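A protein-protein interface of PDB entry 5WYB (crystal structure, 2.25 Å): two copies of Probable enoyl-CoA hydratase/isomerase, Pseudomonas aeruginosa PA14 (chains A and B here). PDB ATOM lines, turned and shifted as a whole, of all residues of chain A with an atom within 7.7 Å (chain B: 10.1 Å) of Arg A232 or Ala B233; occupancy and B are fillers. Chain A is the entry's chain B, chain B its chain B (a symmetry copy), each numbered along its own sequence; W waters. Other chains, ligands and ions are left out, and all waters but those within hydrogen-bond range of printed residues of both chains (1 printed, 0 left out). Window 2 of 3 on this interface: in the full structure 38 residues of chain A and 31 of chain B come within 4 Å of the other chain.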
ATOM      1  N   GLN A 159      -4.948 -18.273 -19.456  1.00  0.00           N
ATOM      2  CA  GLN A 159      -6.026 -18.253 -20.431  1.00  0.00           C
ATOM      3  C   GLN A 159      -6.015 -19.464 -21.341  1.00  0.00           C
ATOM      4  O   GLN A 159      -7.072 -20.012 -21.645  1.00  0.00           O
ATOM      5  CB  GLN A 159      -5.949 -16.977 -21.291  1.00  0.00           C
ATOM      6  CG  GLN A 159      -5.886 -15.682 -20.503  1.00  0.00           C
ATOM      7  CD  GLN A 159      -7.017 -15.563 -19.521  1.00  0.00           C
ATOM      8  OE1 GLN A 159      -8.176 -15.724 -19.876  1.00  0.00           O
ATOM      9  NE2 GLN A 159      -6.686 -15.317 -18.268  1.00  0.00           N
ATOM     10  N   TRP A 163      -8.741 -22.917 -21.559  1.00  0.00           N
ATOM     11  CA  TRP A 163      -9.355 -22.870 -22.874  1.00  0.00           C
ATOM     12  C   TRP A 163      -9.467 -24.281 -23.478  1.00  0.00           C
ATOM     13  O   TRP A 163     -10.455 -24.582 -24.043  1.00  0.00           O
ATOM     14  CB  TRP A 163      -8.655 -21.875 -23.799  1.00  0.00           C
ATOM     15  CG  TRP A 163      -9.364 -21.483 -25.059  1.00  0.00           C
ATOM     16  CD1 TRP A 163      -8.979 -21.744 -26.277  1.00  0.00           C
ATOM     17  CD2 TRP A 163     -10.561 -20.736 -25.175  1.00  0.00           C
ATOM     18  NE1 TRP A 163      -9.827 -21.239 -27.170  1.00  0.00           N
ATOM     19  CE2 TRP A 163     -10.826 -20.603 -26.518  1.00  0.00           C
ATOM     20  CE3 TRP A 163     -11.431 -20.170 -24.272  1.00  0.00           C
ATOM     21  CZ2 TRP A 163     -11.923 -19.927 -26.994  1.00  0.00           C
ATOM     22  CZ3 TRP A 163     -12.516 -19.502 -24.748  1.00  0.00           C
ATOM     23  CH2 TRP A 163     -12.748 -19.385 -26.089  1.00  0.00           C
ATOM     24  N   LEU A 225      -9.911 -17.844 -38.275  1.00  0.00           N
ATOM     25  CA  LEU A 225     -11.321 -18.096 -38.054  1.00  0.00           C
ATOM     26  C   LEU A 225     -11.539 -19.118 -36.926  1.00  0.00           C
ATOM     27  O   LEU A 225     -12.394 -18.973 -36.127  1.00  0.00           O
ATOM     28  CB  LEU A 225     -12.021 -18.553 -39.321  1.00  0.00           C
ATOM     29  CG  LEU A 225     -12.358 -17.527 -40.395  1.00  0.00           C
ATOM     30  CD1 LEU A 225     -13.063 -18.109 -41.586  1.00  0.00           C
ATOM     31  CD2 LEU A 225     -13.171 -16.417 -39.792  1.00  0.00           C
ATOM     32  N   GLN A 227      -9.541 -19.710 -34.398  1.00  0.00           N
ATOM     33  CA  GLN A 227      -9.216 -19.043 -33.143  1.00  0.00           C
ATOM     34  C   GLN A 227     -10.114 -17.842 -32.844  1.00  0.00           C
ATOM     35  O   GLN A 227      -9.830 -17.104 -31.897  1.00  0.00           O
ATOM     36  CB  GLN A 227      -7.753 -18.613 -33.154  1.00  0.00           C
ATOM     37  CG  GLN A 227      -6.809 -19.774 -33.286  1.00  0.00           C
ATOM     38  CD  GLN A 227      -5.411 -19.338 -33.607  1.00  0.00           C
ATOM     39  OE1 GLN A 227      -4.442 -19.987 -33.222  1.00  0.00           O
ATOM     40  NE2 GLN A 227      -5.293 -18.235 -34.329  1.00  0.00           N
ATOM     41  N   GLY A 228     -11.197 -17.654 -33.601  1.00  0.00           N
ATOM     42  CA  GLY A 228     -12.037 -16.481 -33.419  1.00  0.00           C
ATOM     43  C   GLY A 228     -12.619 -16.351 -32.026  1.00  0.00           C
ATOM     44  O   GLY A 228     -12.742 -15.240 -31.506  1.00  0.00           O
ATOM     45  N   ALA A 229     -12.972 -17.473 -31.396  1.00  0.00           N
ATOM     46  CA  ALA A 229     -13.584 -17.400 -30.075  1.00  0.00           C
ATOM     47  C   ALA A 229     -12.622 -16.871 -29.021  1.00  0.00           C
ATOM     48  O   ALA A 229     -13.061 -16.475 -27.939  1.00  0.00           O
ATOM     49  CB  ALA A 229     -14.124 -18.766 -29.662  1.00  0.00           C
ATOM     50  N   ARG A 230     -11.326 -16.841 -29.313  1.00  0.00           N
ATOM     51  CA  ARG A 230     -10.369 -16.332 -28.343  1.00  0.00           C
ATOM     52  C   ARG A 230     -10.484 -14.826 -28.156  1.00  0.00           C
ATOM     53  O   ARG A 230     -10.094 -14.303 -27.106  1.00  0.00           O
ATOM     54  CB  ARG A 230      -8.958 -16.704 -28.775  1.00  0.00           C
ATOM     55  CG  ARG A 230      -8.665 -18.191 -28.699  1.00  0.00           C
ATOM     56  CD  ARG A 230      -7.391 -18.517 -29.441  1.00  0.00           C
ATOM     57  NE  ARG A 230      -6.682 -19.649 -28.853  1.00  0.00           N
ATOM     58  CZ  ARG A 230      -5.489 -20.072 -29.253  1.00  0.00           C
ATOM     59  NH1 ARG A 230      -4.868 -19.467 -30.251  1.00  0.00           N
ATOM     60  NH2 ARG A 230      -4.920 -21.107 -28.662  1.00  0.00           N
ATOM     61  N   GLU A 231     -11.024 -14.119 -29.142  1.00  0.00           N
ATOM     62  CA  GLU A 231     -11.213 -12.686 -29.022  1.00  0.00           C
ATOM     63  C   GLU A 231     -12.669 -12.266 -29.027  1.00  0.00           C
ATOM     64  O   GLU A 231     -12.984 -11.190 -28.515  1.00  0.00           O
ATOM     65  CB  GLU A 231     -10.465 -11.961 -30.145  1.00  0.00           C
ATOM     66  CG  GLU A 231      -9.129 -11.422 -29.682  1.00  0.00           C
ATOM     67  CD  GLU A 231      -8.115 -11.286 -30.796  1.00  0.00           C
ATOM     68  OE1 GLU A 231      -8.481 -11.490 -31.975  1.00  0.00           O
ATOM     69  OE2 GLU A 231      -6.946 -10.976 -30.485  1.00  0.00           O
ATOM     70  N   ARG A 232     -13.565 -13.102 -29.534  1.00  0.00           N
ATOM     71  CA  ARG A 232     -14.950 -12.698 -29.693  1.00  0.00           C
ATOM     72  C   ARG A 232     -15.802 -13.942 -29.886  1.00  0.00           C
ATOM     73  O   ARG A 232     -15.363 -14.913 -30.499  1.00  0.00           O
ATOM     74  CB  ARG A 232     -15.092 -11.747 -30.882  1.00  0.00           C
ATOM     75  CG  ARG A 232     -16.330 -10.911 -30.876  1.00  0.00           C
ATOM     76  CD  ARG A 232     -16.120  -9.736 -31.808  1.00  0.00           C
ATOM     77  NE  ARG A 232     -16.146 -10.128 -33.213  1.00  0.00           N
ATOM     78  CZ  ARG A 232     -15.363  -9.598 -34.144  1.00  0.00           C
ATOM     79  NH1 ARG A 232     -14.477  -8.668 -33.815  1.00  0.00           N
ATOM     80  NH2 ARG A 232     -15.454 -10.005 -35.401  1.00  0.00           N
ATOM     81  N   ALA A 233     -17.028 -13.883 -29.376  1.00  0.00           N
ATOM     82  CA  ALA A 233     -17.918 -15.029 -29.390  1.00  0.00           C
ATOM     83  C   ALA A 233     -18.053 -15.597 -30.802  1.00  0.00           C
ATOM     84  O   ALA A 233     -17.932 -14.867 -31.787  1.00  0.00           O
ATOM     85  CB  ALA A 233     -19.288 -14.641 -28.852  1.00  0.00           C
ATOM     86  N   PRO A 234     -18.303 -16.904 -30.924  1.00  0.00           N
ATOM     87  CA  PRO A 234     -18.273 -17.535 -32.254  1.00  0.00           C
ATOM     88  C   PRO A 234     -19.327 -17.015 -33.213  1.00  0.00           C
ATOM     89  O   PRO A 234     -19.069 -16.949 -34.419  1.00  0.00           O
ATOM     90  CB  PRO A 234     -18.496 -19.024 -31.935  1.00  0.00           C
ATOM     91  CG  PRO A 234     -18.144 -19.170 -30.512  1.00  0.00           C
ATOM     92  CD  PRO A 234     -18.502 -17.893 -29.850  1.00  0.00           C
ATOM     93  N   ASN A 235     -20.518 -16.673 -32.725  1.00  0.00           N
ATOM     94  CA  ASN A 235     -21.577 -16.248 -33.637  1.00  0.00           C
ATOM     95  C   ASN A 235     -21.230 -14.943 -34.339  1.00  0.00           C
ATOM     96  O   ASN A 235     -21.724 -14.680 -35.439  1.00  0.00           O
ATOM     97  CB  ASN A 235     -22.897 -16.099 -32.890  1.00  0.00           C
ATOM     98  CG  ASN A 235     -23.430 -17.416 -32.386  1.00  0.00           C
ATOM     99  OD1 ASN A 235     -22.766 -18.445 -32.492  1.00  0.00           O
ATOM    100  ND2 ASN A 235     -24.638 -17.399 -31.834  1.00  0.00           N
ATOM    101  N   THR A 236     -20.377 -14.122 -33.731  1.00  0.00           N
ATOM    102  CA  THR A 236     -20.005 -12.853 -34.330  1.00  0.00           C
ATOM    103  C   THR A 236     -19.120 -13.015 -35.555  1.00  0.00           C
ATOM    104  O   THR A 236     -18.926 -12.036 -36.285  1.00  0.00           O
ATOM    105  CB  THR A 236     -19.308 -11.979 -33.290  1.00  0.00           C
ATOM    106  OG1 THR A 236     -17.934 -12.348 -33.195  1.00  0.00           O
ATOM    107  CG2 THR A 236     -19.955 -12.167 -31.940  1.00  0.00           C
ATOM    108  N   TRP A 237     -18.593 -14.214 -35.812  1.00  0.00           N
ATOM    109  CA  TRP A 237     -17.698 -14.443 -36.937  1.00  0.00           C
ATOM    110  C   TRP A 237     -18.382 -15.083 -38.131  1.00  0.00           C
ATOM    111  O   TRP A 237     -17.765 -15.179 -39.195  1.00  0.00           O
ATOM    112  CB  TRP A 237     -16.525 -15.334 -36.515  1.00  0.00           C
ATOM    113  CG  TRP A 237     -15.795 -14.833 -35.336  1.00  0.00           C
ATOM    114  CD1 TRP A 237     -16.048 -15.126 -34.035  1.00  0.00           C
ATOM    115  CD2 TRP A 237     -14.682 -13.938 -35.337  1.00  0.00           C
ATOM    116  NE1 TRP A 237     -15.162 -14.472 -33.220  1.00  0.00           N
ATOM    117  CE2 TRP A 237     -14.310 -13.736 -33.999  1.00  0.00           C
ATOM    118  CE3 TRP A 237     -13.963 -13.286 -36.340  1.00  0.00           C
ATOM    119  CZ2 TRP A 237     -13.256 -12.910 -33.637  1.00  0.00           C
ATOM    120  CZ3 TRP A 237     -12.916 -12.466 -35.980  1.00  0.00           C
ATOM    121  CH2 TRP A 237     -12.571 -12.285 -34.641  1.00  0.00           C
ATOM    122  N   LEU A 238     -19.622 -15.533 -37.979  1.00  0.00           N
ATOM    123  CA  LEU A 238     -20.268 -16.271 -39.060  1.00  0.00           C
ATOM    124  C   LEU A 238     -20.377 -15.470 -40.349  1.00  0.00           C
ATOM    125  O   LEU A 238     -20.097 -16.041 -41.417  1.00  0.00           O
ATOM    126  CB  LEU A 238     -21.647 -16.766 -38.605  1.00  0.00           C
ATOM    127  CG  LEU A 238     -21.632 -17.851 -37.527  1.00  0.00           C
ATOM    128  CD1 LEU A 238     -23.042 -18.255 -37.157  1.00  0.00           C
ATOM    129  CD2 LEU A 238     -20.828 -19.070 -37.990  1.00  0.00           C
ATOM    130  N   PRO A 239     -20.767 -14.189 -40.345  1.00  0.00           N
ATOM    131  CA  PRO A 239     -20.749 -13.453 -41.615  1.00  0.00           C
ATOM    132  C   PRO A 239     -19.351 -13.323 -42.187  1.00  0.00           C
ATOM    133  O   PRO A 239     -19.179 -13.407 -43.407  1.00  0.00           O
ATOM    134  CB  PRO A 239     -21.374 -12.096 -41.248  1.00  0.00           C
ATOM    135  CG  PRO A 239     -21.248 -11.996 -39.784  1.00  0.00           C
ATOM    136  CD  PRO A 239     -21.357 -13.382 -39.263  1.00  0.00           C
ATOM    137  N   GLU A 240     -18.367 -13.165 -41.338  1.00  0.00           N
ATOM    138  CA  GLU A 240     -17.015 -13.132 -41.799  1.00  0.00           C
ATOM    139  C   GLU A 240     -16.565 -14.449 -42.413  1.00  0.00           C
ATOM    140  O   GLU A 240     -15.732 -14.465 -43.246  1.00  0.00           O
ATOM    141  CB  GLU A 240     -16.005 -12.704 -40.780  1.00  0.00           C
ATOM    142  CG  GLU A 240     -14.886 -11.993 -41.490  1.00  0.00           C
ATOM    143  CD  GLU A 240     -13.572 -12.076 -40.810  1.00  0.00           C
ATOM    144  OE1 GLU A 240     -13.533 -12.056 -39.591  1.00  0.00           O
ATOM    145  OE2 GLU A 240     -12.575 -12.118 -41.508  1.00  0.00           O
ATOM    146  N   TRP B 163     -20.647 -24.840 -19.909  1.00  0.00           N
ATOM    147  CA  TRP B 163     -19.308 -24.286 -19.813  1.00  0.00           C
ATOM    148  C   TRP B 163     -18.268 -25.402 -19.603  1.00  0.00           C
ATOM    149  O   TRP B 163     -17.251 -25.350 -20.193  1.00  0.00           O
ATOM    150  CB  TRP B 163     -19.218 -23.177 -18.767  1.00  0.00           C
ATOM    151  CG  TRP B 163     -18.002 -22.302 -18.786  1.00  0.00           C
ATOM    152  CD1 TRP B 163     -17.088 -22.227 -17.859  1.00  0.00           C
ATOM    153  CD2 TRP B 163     -17.624 -21.377 -19.790  1.00  0.00           C
ATOM    154  NE1 TRP B 163     -16.147 -21.340 -18.179  1.00  0.00           N
ATOM    155  CE2 TRP B 163     -16.451 -20.791 -19.376  1.00  0.00           C
ATOM    156  CE3 TRP B 163     -18.166 -20.992 -20.995  1.00  0.00           C
ATOM    157  CZ2 TRP B 163     -15.799 -19.834 -20.116  1.00  0.00           C
ATOM    158  CZ3 TRP B 163     -17.517 -20.046 -21.724  1.00  0.00           C
ATOM    159  CH2 TRP B 163     -16.353 -19.479 -21.282  1.00  0.00           C
ATOM    160  N   PRO B 224      -9.113 -15.380 -10.420  1.00  0.00           N
ATOM    161  CA  PRO B 224      -9.975 -14.572 -11.292  1.00  0.00           C
ATOM    162  C   PRO B 224      -9.511 -14.588 -12.737  1.00  0.00           C
ATOM    163  O   PRO B 224     -10.315 -14.506 -13.628  1.00  0.00           O
ATOM    164  CB  PRO B 224      -9.850 -13.187 -10.725  1.00  0.00           C
ATOM    165  CG  PRO B 224      -9.608 -13.392  -9.317  1.00  0.00           C
ATOM    166  CD  PRO B 224      -8.590 -14.453  -9.337  1.00  0.00           C
ATOM    167  N   LEU B 225      -8.209 -14.673 -12.947  1.00  0.00           N
ATOM    168  CA  LEU B 225      -7.660 -14.755 -14.287  1.00  0.00           C
ATOM    169  C   LEU B 225      -8.127 -16.030 -15.008  1.00  0.00           C
ATOM    170  O   LEU B 225      -8.442 -16.008 -16.144  1.00  0.00           O
ATOM    171  CB  LEU B 225      -6.145 -14.675 -14.284  1.00  0.00           C
ATOM    172  CG  LEU B 225      -5.472 -13.324 -14.075  1.00  0.00           C
ATOM    173  CD1 LEU B 225      -3.972 -13.386 -14.112  1.00  0.00           C
ATOM    174  CD2 LEU B 225      -5.984 -12.345 -15.091  1.00  0.00           C
ATOM    175  N   ILE B 226      -8.161 -17.140 -14.303  1.00  0.00           N
ATOM    176  CA  ILE B 226      -8.606 -18.393 -14.901  1.00  0.00           C
ATOM    177  C   ILE B 226     -10.069 -18.294 -15.309  1.00  0.00           C
ATOM    178  O   ILE B 226     -10.455 -18.736 -16.396  1.00  0.00           O
ATOM    179  CB  ILE B 226      -8.357 -19.570 -13.936  1.00  0.00           C
ATOM    180  CG1 ILE B 226      -6.863 -19.720 -13.653  1.00  0.00           C
ATOM    181  CG2 ILE B 226      -8.884 -20.855 -14.522  1.00  0.00           C
ATOM    182  CD1 ILE B 226      -6.529 -20.861 -12.720  1.00  0.00           C
ATOM    183  N   GLN B 227     -10.898 -17.692 -14.467  1.00  0.00           N
ATOM    184  CA  GLN B 227     -12.307 -17.512 -14.795  1.00  0.00           C
ATOM    185  C   GLN B 227     -12.564 -16.338 -15.741  1.00  0.00           C
ATOM    186  O   GLN B 227     -13.727 -15.988 -15.958  1.00  0.00           O
ATOM    187  CB  GLN B 227     -13.113 -17.338 -13.513  1.00  0.00           C
ATOM    188  CG  GLN B 227     -13.028 -18.533 -12.607  1.00  0.00           C
ATOM    189  CD  GLN B 227     -13.554 -18.246 -11.233  1.00  0.00           C
ATOM    190  OE1 GLN B 227     -14.083 -19.128 -10.561  1.00  0.00           O
ATOM    191  NE2 GLN B 227     -13.403 -17.006 -10.796  1.00  0.00           N
ATOM    192  N   GLY B 228     -11.516 -15.753 -16.328  1.00  0.00           N
ATOM    193  CA  GLY B 228     -11.695 -14.579 -17.166  1.00  0.00           C
ATOM    194  C   GLY B 228     -12.616 -14.800 -18.349  1.00  0.00           C
ATOM    195  O   GLY B 228     -13.376 -13.903 -18.721  1.00  0.00           O
ATOM    196  N   ALA B 229     -12.578 -15.993 -18.947  1.00  0.00           N
ATOM    197  CA  ALA B 229     -13.407 -16.241 -20.121  1.00  0.00           C
ATOM    198  C   ALA B 229     -14.892 -16.228 -19.792  1.00  0.00           C
ATOM    199  O   ALA B 229     -15.717 -16.126 -20.703  1.00  0.00           O
ATOM    200  CB  ALA B 229     -13.020 -17.564 -20.776  1.00  0.00           C
ATOM    201  N   ARG B 230     -15.253 -16.314 -18.517  1.00  0.00           N
ATOM    202  CA  ARG B 230     -16.662 -16.292 -18.150  1.00  0.00           C
ATOM    203  C   ARG B 230     -17.290 -14.922 -18.360  1.00  0.00           C
ATOM    204  O   ARG B 230     -18.510 -14.822 -18.531  1.00  0.00           O
ATOM    205  CB  ARG B 230     -16.819 -16.729 -16.701  1.00  0.00           C
ATOM    206  CG  ARG B 230     -16.494 -18.191 -16.463  1.00  0.00           C
ATOM    207  CD  ARG B 230     -16.352 -18.467 -14.985  1.00  0.00           C
ATOM    208  NE  ARG B 230     -16.759 -19.823 -14.632  1.00  0.00           N
ATOM    209  CZ  ARG B 230     -16.825 -20.283 -13.390  1.00  0.00           C
ATOM    210  NH1 ARG B 230     -16.504 -19.503 -12.372  1.00  0.00           N
ATOM    211  NH2 ARG B 230     -17.205 -21.527 -13.162  1.00  0.00           N
ATOM    212  N   GLU B 231     -16.485 -13.866 -18.368  1.00  0.00           N
ATOM    213  CA  GLU B 231     -17.000 -12.532 -18.609  1.00  0.00           C
ATOM    214  C   GLU B 231     -16.481 -11.906 -19.888  1.00  0.00           C
ATOM    215  O   GLU B 231     -17.134 -11.009 -20.424  1.00  0.00           O
ATOM    216  CB  GLU B 231     -16.675 -11.620 -17.423  1.00  0.00           C
ATOM    217  CG  GLU B 231     -17.851 -11.472 -16.481  1.00  0.00           C
ATOM    218  CD  GLU B 231     -17.447 -11.156 -15.058  1.00  0.00           C
ATOM    219  OE1 GLU B 231     -16.244 -10.920 -14.809  1.00  0.00           O
ATOM    220  OE2 GLU B 231     -18.342 -11.149 -14.187  1.00  0.00           O
ATOM    221  N   ARG B 232     -15.365 -12.388 -20.418  1.00  0.00           N
ATOM    222  CA  ARG B 232     -14.746 -11.740 -21.561  1.00  0.00           C
ATOM    223  C   ARG B 232     -13.764 -12.710 -22.199  1.00  0.00           C
ATOM    224  O   ARG B 232     -13.123 -13.498 -21.507  1.00  0.00           O
ATOM    225  CB  ARG B 232     -14.041 -10.455 -21.125  1.00  0.00           C
ATOM    226  CG  ARG B 232     -13.776  -9.478 -22.223  1.00  0.00           C
ATOM    227  CD  ARG B 232     -13.521  -8.119 -21.606  1.00  0.00           C
ATOM    228  NE  ARG B 232     -12.222  -8.043 -20.947  1.00  0.00           N
ATOM    229  CZ  ARG B 232     -12.002  -7.379 -19.818  1.00  0.00           C
ATOM    230  NH1 ARG B 232     -12.999  -6.751 -19.212  1.00  0.00           N
ATOM    231  NH2 ARG B 232     -10.788  -7.352 -19.287  1.00  0.00           N
ATOM    232  N   ALA B 233     -13.645 -12.619 -23.519  1.00  0.00           N
ATOM    233  CA  ALA B 233     -12.827 -13.548 -24.278  1.00  0.00           C
ATOM    234  C   ALA B 233     -11.410 -13.617 -23.709  1.00  0.00           C
ATOM    235  O   ALA B 233     -10.915 -12.643 -23.139  1.00  0.00           O
ATOM    236  CB  ALA B 233     -12.780 -13.135 -25.743  1.00  0.00           C
ATOM    237  N   PRO B 234     -10.739 -14.763 -23.854  1.00  0.00           N
ATOM    238  CA  PRO B 234      -9.443 -14.942 -23.179  1.00  0.00           C
ATOM    239  C   PRO B 234      -8.361 -13.988 -23.647  1.00  0.00           C
ATOM    240  O   PRO B 234      -7.514 -13.590 -22.841  1.00  0.00           O
ATOM    241  CB  PRO B 234      -9.081 -16.401 -23.509  1.00  0.00           C
ATOM    242  CG  PRO B 234     -10.355 -17.039 -23.884  1.00  0.00           C
ATOM    243  CD  PRO B 234     -11.181 -15.993 -24.533  1.00  0.00           C
ATOM    244  N   ASN B 235      -8.338 -13.631 -24.930  1.00  0.00           N
ATOM    245  CA  ASN B 235      -7.258 -12.781 -25.424  1.00  0.00           C
ATOM    246  C   ASN B 235      -7.299 -11.394 -24.798  1.00  0.00           C
ATOM    247  O   ASN B 235      -6.266 -10.725 -24.705  1.00  0.00           O
ATOM    248  CB  ASN B 235      -7.322 -12.666 -26.942  1.00  0.00           C
ATOM    249  CG  ASN B 235      -7.030 -13.972 -27.635  1.00  0.00           C
ATOM    250  OD1 ASN B 235      -6.884 -15.007 -26.990  1.00  0.00           O
ATOM    251  ND2 ASN B 235      -6.938 -13.937 -28.961  1.00  0.00           N
ATOM    252  N   THR B 236      -8.473 -10.951 -24.354  1.00  0.00           N
ATOM    253  CA  THR B 236      -8.596  -9.633 -23.756  1.00  0.00           C
ATOM    254  C   THR B 236      -7.939  -9.542 -22.388  1.00  0.00           C
ATOM    255  O   THR B 236      -7.773  -8.428 -21.879  1.00  0.00           O
ATOM    256  CB  THR B 236     -10.072  -9.251 -23.657  1.00  0.00           C
ATOM    257  OG1 THR B 236     -10.645  -9.844 -22.494  1.00  0.00           O
ATOM    258  CG2 THR B 236     -10.817  -9.747 -24.872  1.00  0.00           C
ATOM    259  N   TRP B 237      -7.549 -10.668 -21.788  1.00  0.00           N
ATOM    260  CA  TRP B 237      -6.954 -10.672 -20.458  1.00  0.00           C
ATOM    261  C   TRP B 237      -5.441 -10.789 -20.475  1.00  0.00           C
ATOM    262  O   TRP B 237      -4.818 -10.644 -19.421  1.00  0.00           O
ATOM    263  CB  TRP B 237      -7.521 -11.825 -19.623  1.00  0.00           C
ATOM    264  CG  TRP B 237      -8.994 -11.840 -19.557  1.00  0.00           C
ATOM    265  CD1 TRP B 237      -9.841 -12.481 -20.402  1.00  0.00           C
ATOM    266  CD2 TRP B 237      -9.814 -11.178 -18.593  1.00  0.00           C
ATOM    267  NE1 TRP B 237     -11.141 -12.264 -20.026  1.00  0.00           N
ATOM    268  CE2 TRP B 237     -11.148 -11.466 -18.914  1.00  0.00           C
ATOM    269  CE3 TRP B 237      -9.548 -10.367 -17.488  1.00  0.00           C
ATOM    270  CZ2 TRP B 237     -12.214 -10.973 -18.174  1.00  0.00           C
ATOM    271  CZ3 TRP B 237     -10.606  -9.879 -16.753  1.00  0.00           C
ATOM    272  CH2 TRP B 237     -11.923 -10.183 -17.098  1.00  0.00           C
ATOM    273  N   LEU B 238      -4.845 -11.062 -21.630  1.00  0.00           N
ATOM    274  CA  LEU B 238      -3.406 -11.313 -21.666  1.00  0.00           C
ATOM    275  C   LEU B 238      -2.583 -10.142 -21.150  1.00  0.00           C
ATOM    276  O   LEU B 238      -1.636 -10.387 -20.384  1.00  0.00           O
ATOM    277  CB  LEU B 238      -2.978 -11.699 -23.087  1.00  0.00           C
ATOM    278  CG  LEU B 238      -3.487 -13.055 -23.578  1.00  0.00           C
ATOM    279  CD1 LEU B 238      -3.007 -13.326 -24.987  1.00  0.00           C
ATOM    280  CD2 LEU B 238      -3.046 -14.179 -22.637  1.00  0.00           C
ATOM    281  N   PRO B 239      -2.858  -8.881 -21.511  1.00  0.00           N
ATOM    282  CA  PRO B 239      -2.084  -7.797 -20.892  1.00  0.00           C
ATOM    283  C   PRO B 239      -2.297  -7.718 -19.393  1.00  0.00           C
ATOM    284  O   PRO B 239      -1.347  -7.443 -18.654  1.00  0.00           O
ATOM    285  CB  PRO B 239      -2.576  -6.543 -21.634  1.00  0.00           C
ATOM    286  CG  PRO B 239      -3.866  -6.927 -22.228  1.00  0.00           C
ATOM    287  CD  PRO B 239      -3.758  -8.371 -22.559  1.00  0.00           C
ATOM    288  N   GLU B 240      -3.495  -7.992 -18.943  1.00  0.00           N
ATOM    289  CA  GLU B 240      -3.744  -8.031 -17.535  1.00  0.00           C
ATOM    290  C   GLU B 240      -2.985  -9.144 -16.828  1.00  0.00           C
ATOM    291  O   GLU B 240      -2.676  -9.030 -15.697  1.00  0.00           O
ATOM    292  CB  GLU B 240      -5.188  -8.110 -17.147  1.00  0.00           C
ATOM    293  CG  GLU B 240      -5.365  -7.399 -15.834  1.00  0.00           C
ATOM    294  CD  GLU B 240      -6.491  -7.898 -15.007  1.00  0.00           C
ATOM    295  OE1 GLU B 240      -7.514  -8.267 -15.561  1.00  0.00           O
ATOM    296  OE2 GLU B 240      -6.358  -7.877 -13.797  1.00  0.00           O
HETATM  297  O   HOH W   1      -7.063 -15.427 -31.824  1.00  0.00           O
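The side-chain amide nitrogen of Gln A159 is in hydrogen-bond range of the backbone carbonyl oxygen of Leu B225 (2.8 Å). The side-chain carboxylate (OE2) of Glu A231 is in hydrogen-bond range of the side-chain amide nitrogen (ND2) of Asn B235 (3.3 Å). N of Pro B234 sits close to O of Arg A230 (3.3 Å). The backbone carbonyl oxygen of Arg A230 is in hydrogen-bond range of the backbone NH of Asn B235.
The backbone carbonyl oxygen (O) of Gly B228 sits at hydrogen-bond distance from the indole nitrogen (NE1) of Trp B237, 3.1 Å away. O of Arg B232 lies within hydrogen-bond range of NE1 of Trp B237, 2.8 Å away. OE1 of Gln A227 sits at hydrogen-bond distance from NH1 of Arg A230, at 3.0 Å. The backbone carbonyl oxygen (O) of Ala B233 lies close to the indole nitrogen (NE1) of Trp B237 (3.1 Å). The guanidinium group (NE) of Arg A232 is in hydrogen-bond range of the side-chain hydroxyl (OG1) of Thr A236 (2.9 Å). The backbone carbonyl oxygen of Ala B233 sits at hydrogen-bond distance from the side-chain hydroxyl of Thr B236.
O of Pro B234 touches CG of Gln A159, at 3.5 Å. Gln A159 touches Trp B237 (OE1 to CD1, 3.7 Å). Gln A159 touches Leu B238. Trp A163 touches Pro B234. Ala A229 touches Pro B234 (O to CD, 3.9 Å). O of Arg A230 touches CB of Ala B233 (3.2 Å). Glu A231 touches Ala B233. N of Arg A232 touches CB of Ala B233, 3.9 Å away.
Arg A232 touches one residue of chain B. Printed residues of chain A within 4 Å of Ala B233: Arg A230, Glu A231 and Arg A232. No residue of chain B comes within 4 Å of Gly A228. No residue of chain B comes within 4 Å of Ala A233. No residue of chain B comes within 4 Å of Pro A234. Pro B234 touches just these residues of chain A: Gln A159, Trp A163, Ala A229 and Arg A230. Printed residues of chain A within 4 Å of Trp B237: Gln A159 (3.7 Å). Printed residues of chain A within 4 Å of Leu B225: Gln A159. Of the printed residues of chain B, Glu A231 touches Ala B233 and Asn B235. Of the printed residues of chain A, Leu B238 touches Gln A159 (3.9 Å). Asn A235 touches none of the printed residues of chain B. Glu A240 touches none of the printed residues of chain B. The nearest residue of chain B that does not touch Arg A232 is Pro B234 (6.2 Å). The nearest printed residue of chain A that does not touch Ala B233 is Ala A229 (4.01 Å).
Of the 18 printed residues of chain B, 6 touch a printed residue of chain A. Printed residues of chain B that touch a printed residue of chain A: Leu B225, Ala B233, Pro B234, Asn B235, Trp B237 and Leu B238. Hydrophobic or aromatic side chains of chain B that line the printed part of chain A: Ala B233, Pro B234, Trp B237 and Leu B238. Of the 17 printed residues of chain A, 6 touch a printed residue of chain B. Among the printed residues, no Asp or Glu carboxylate lies within 4 Å of a Lys or Arg side-chain nitrogen of the other chain.
Trp A163 touches Pro B234, but with the chains exchanged Pro A234 does not touch Trp B163 (8.5 Å). Arg A230 touches Ala B233, but with the chains exchanged Ala A233 does not touch Arg B230 (10.4 Å). Arg A230 touches Asn B235, but with the chains exchanged Asn A235 does not touch Arg B230 (14.5 Å). Arg A232 touches Ala B233, but with the chains exchanged Ala A233 does not touch Arg B232 (8.0 Å). Of the 12 pairs that touch across the chains among the printed residues, none has its exchanged pair printed and touching as well.
Water W1 lies within hydrogen-bond range of the side-chain amide nitrogen (ND2) of Asn B235 (3.2 Å) and the backbone carbonyl oxygen (O) of Gln A227 (3.2 Å).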
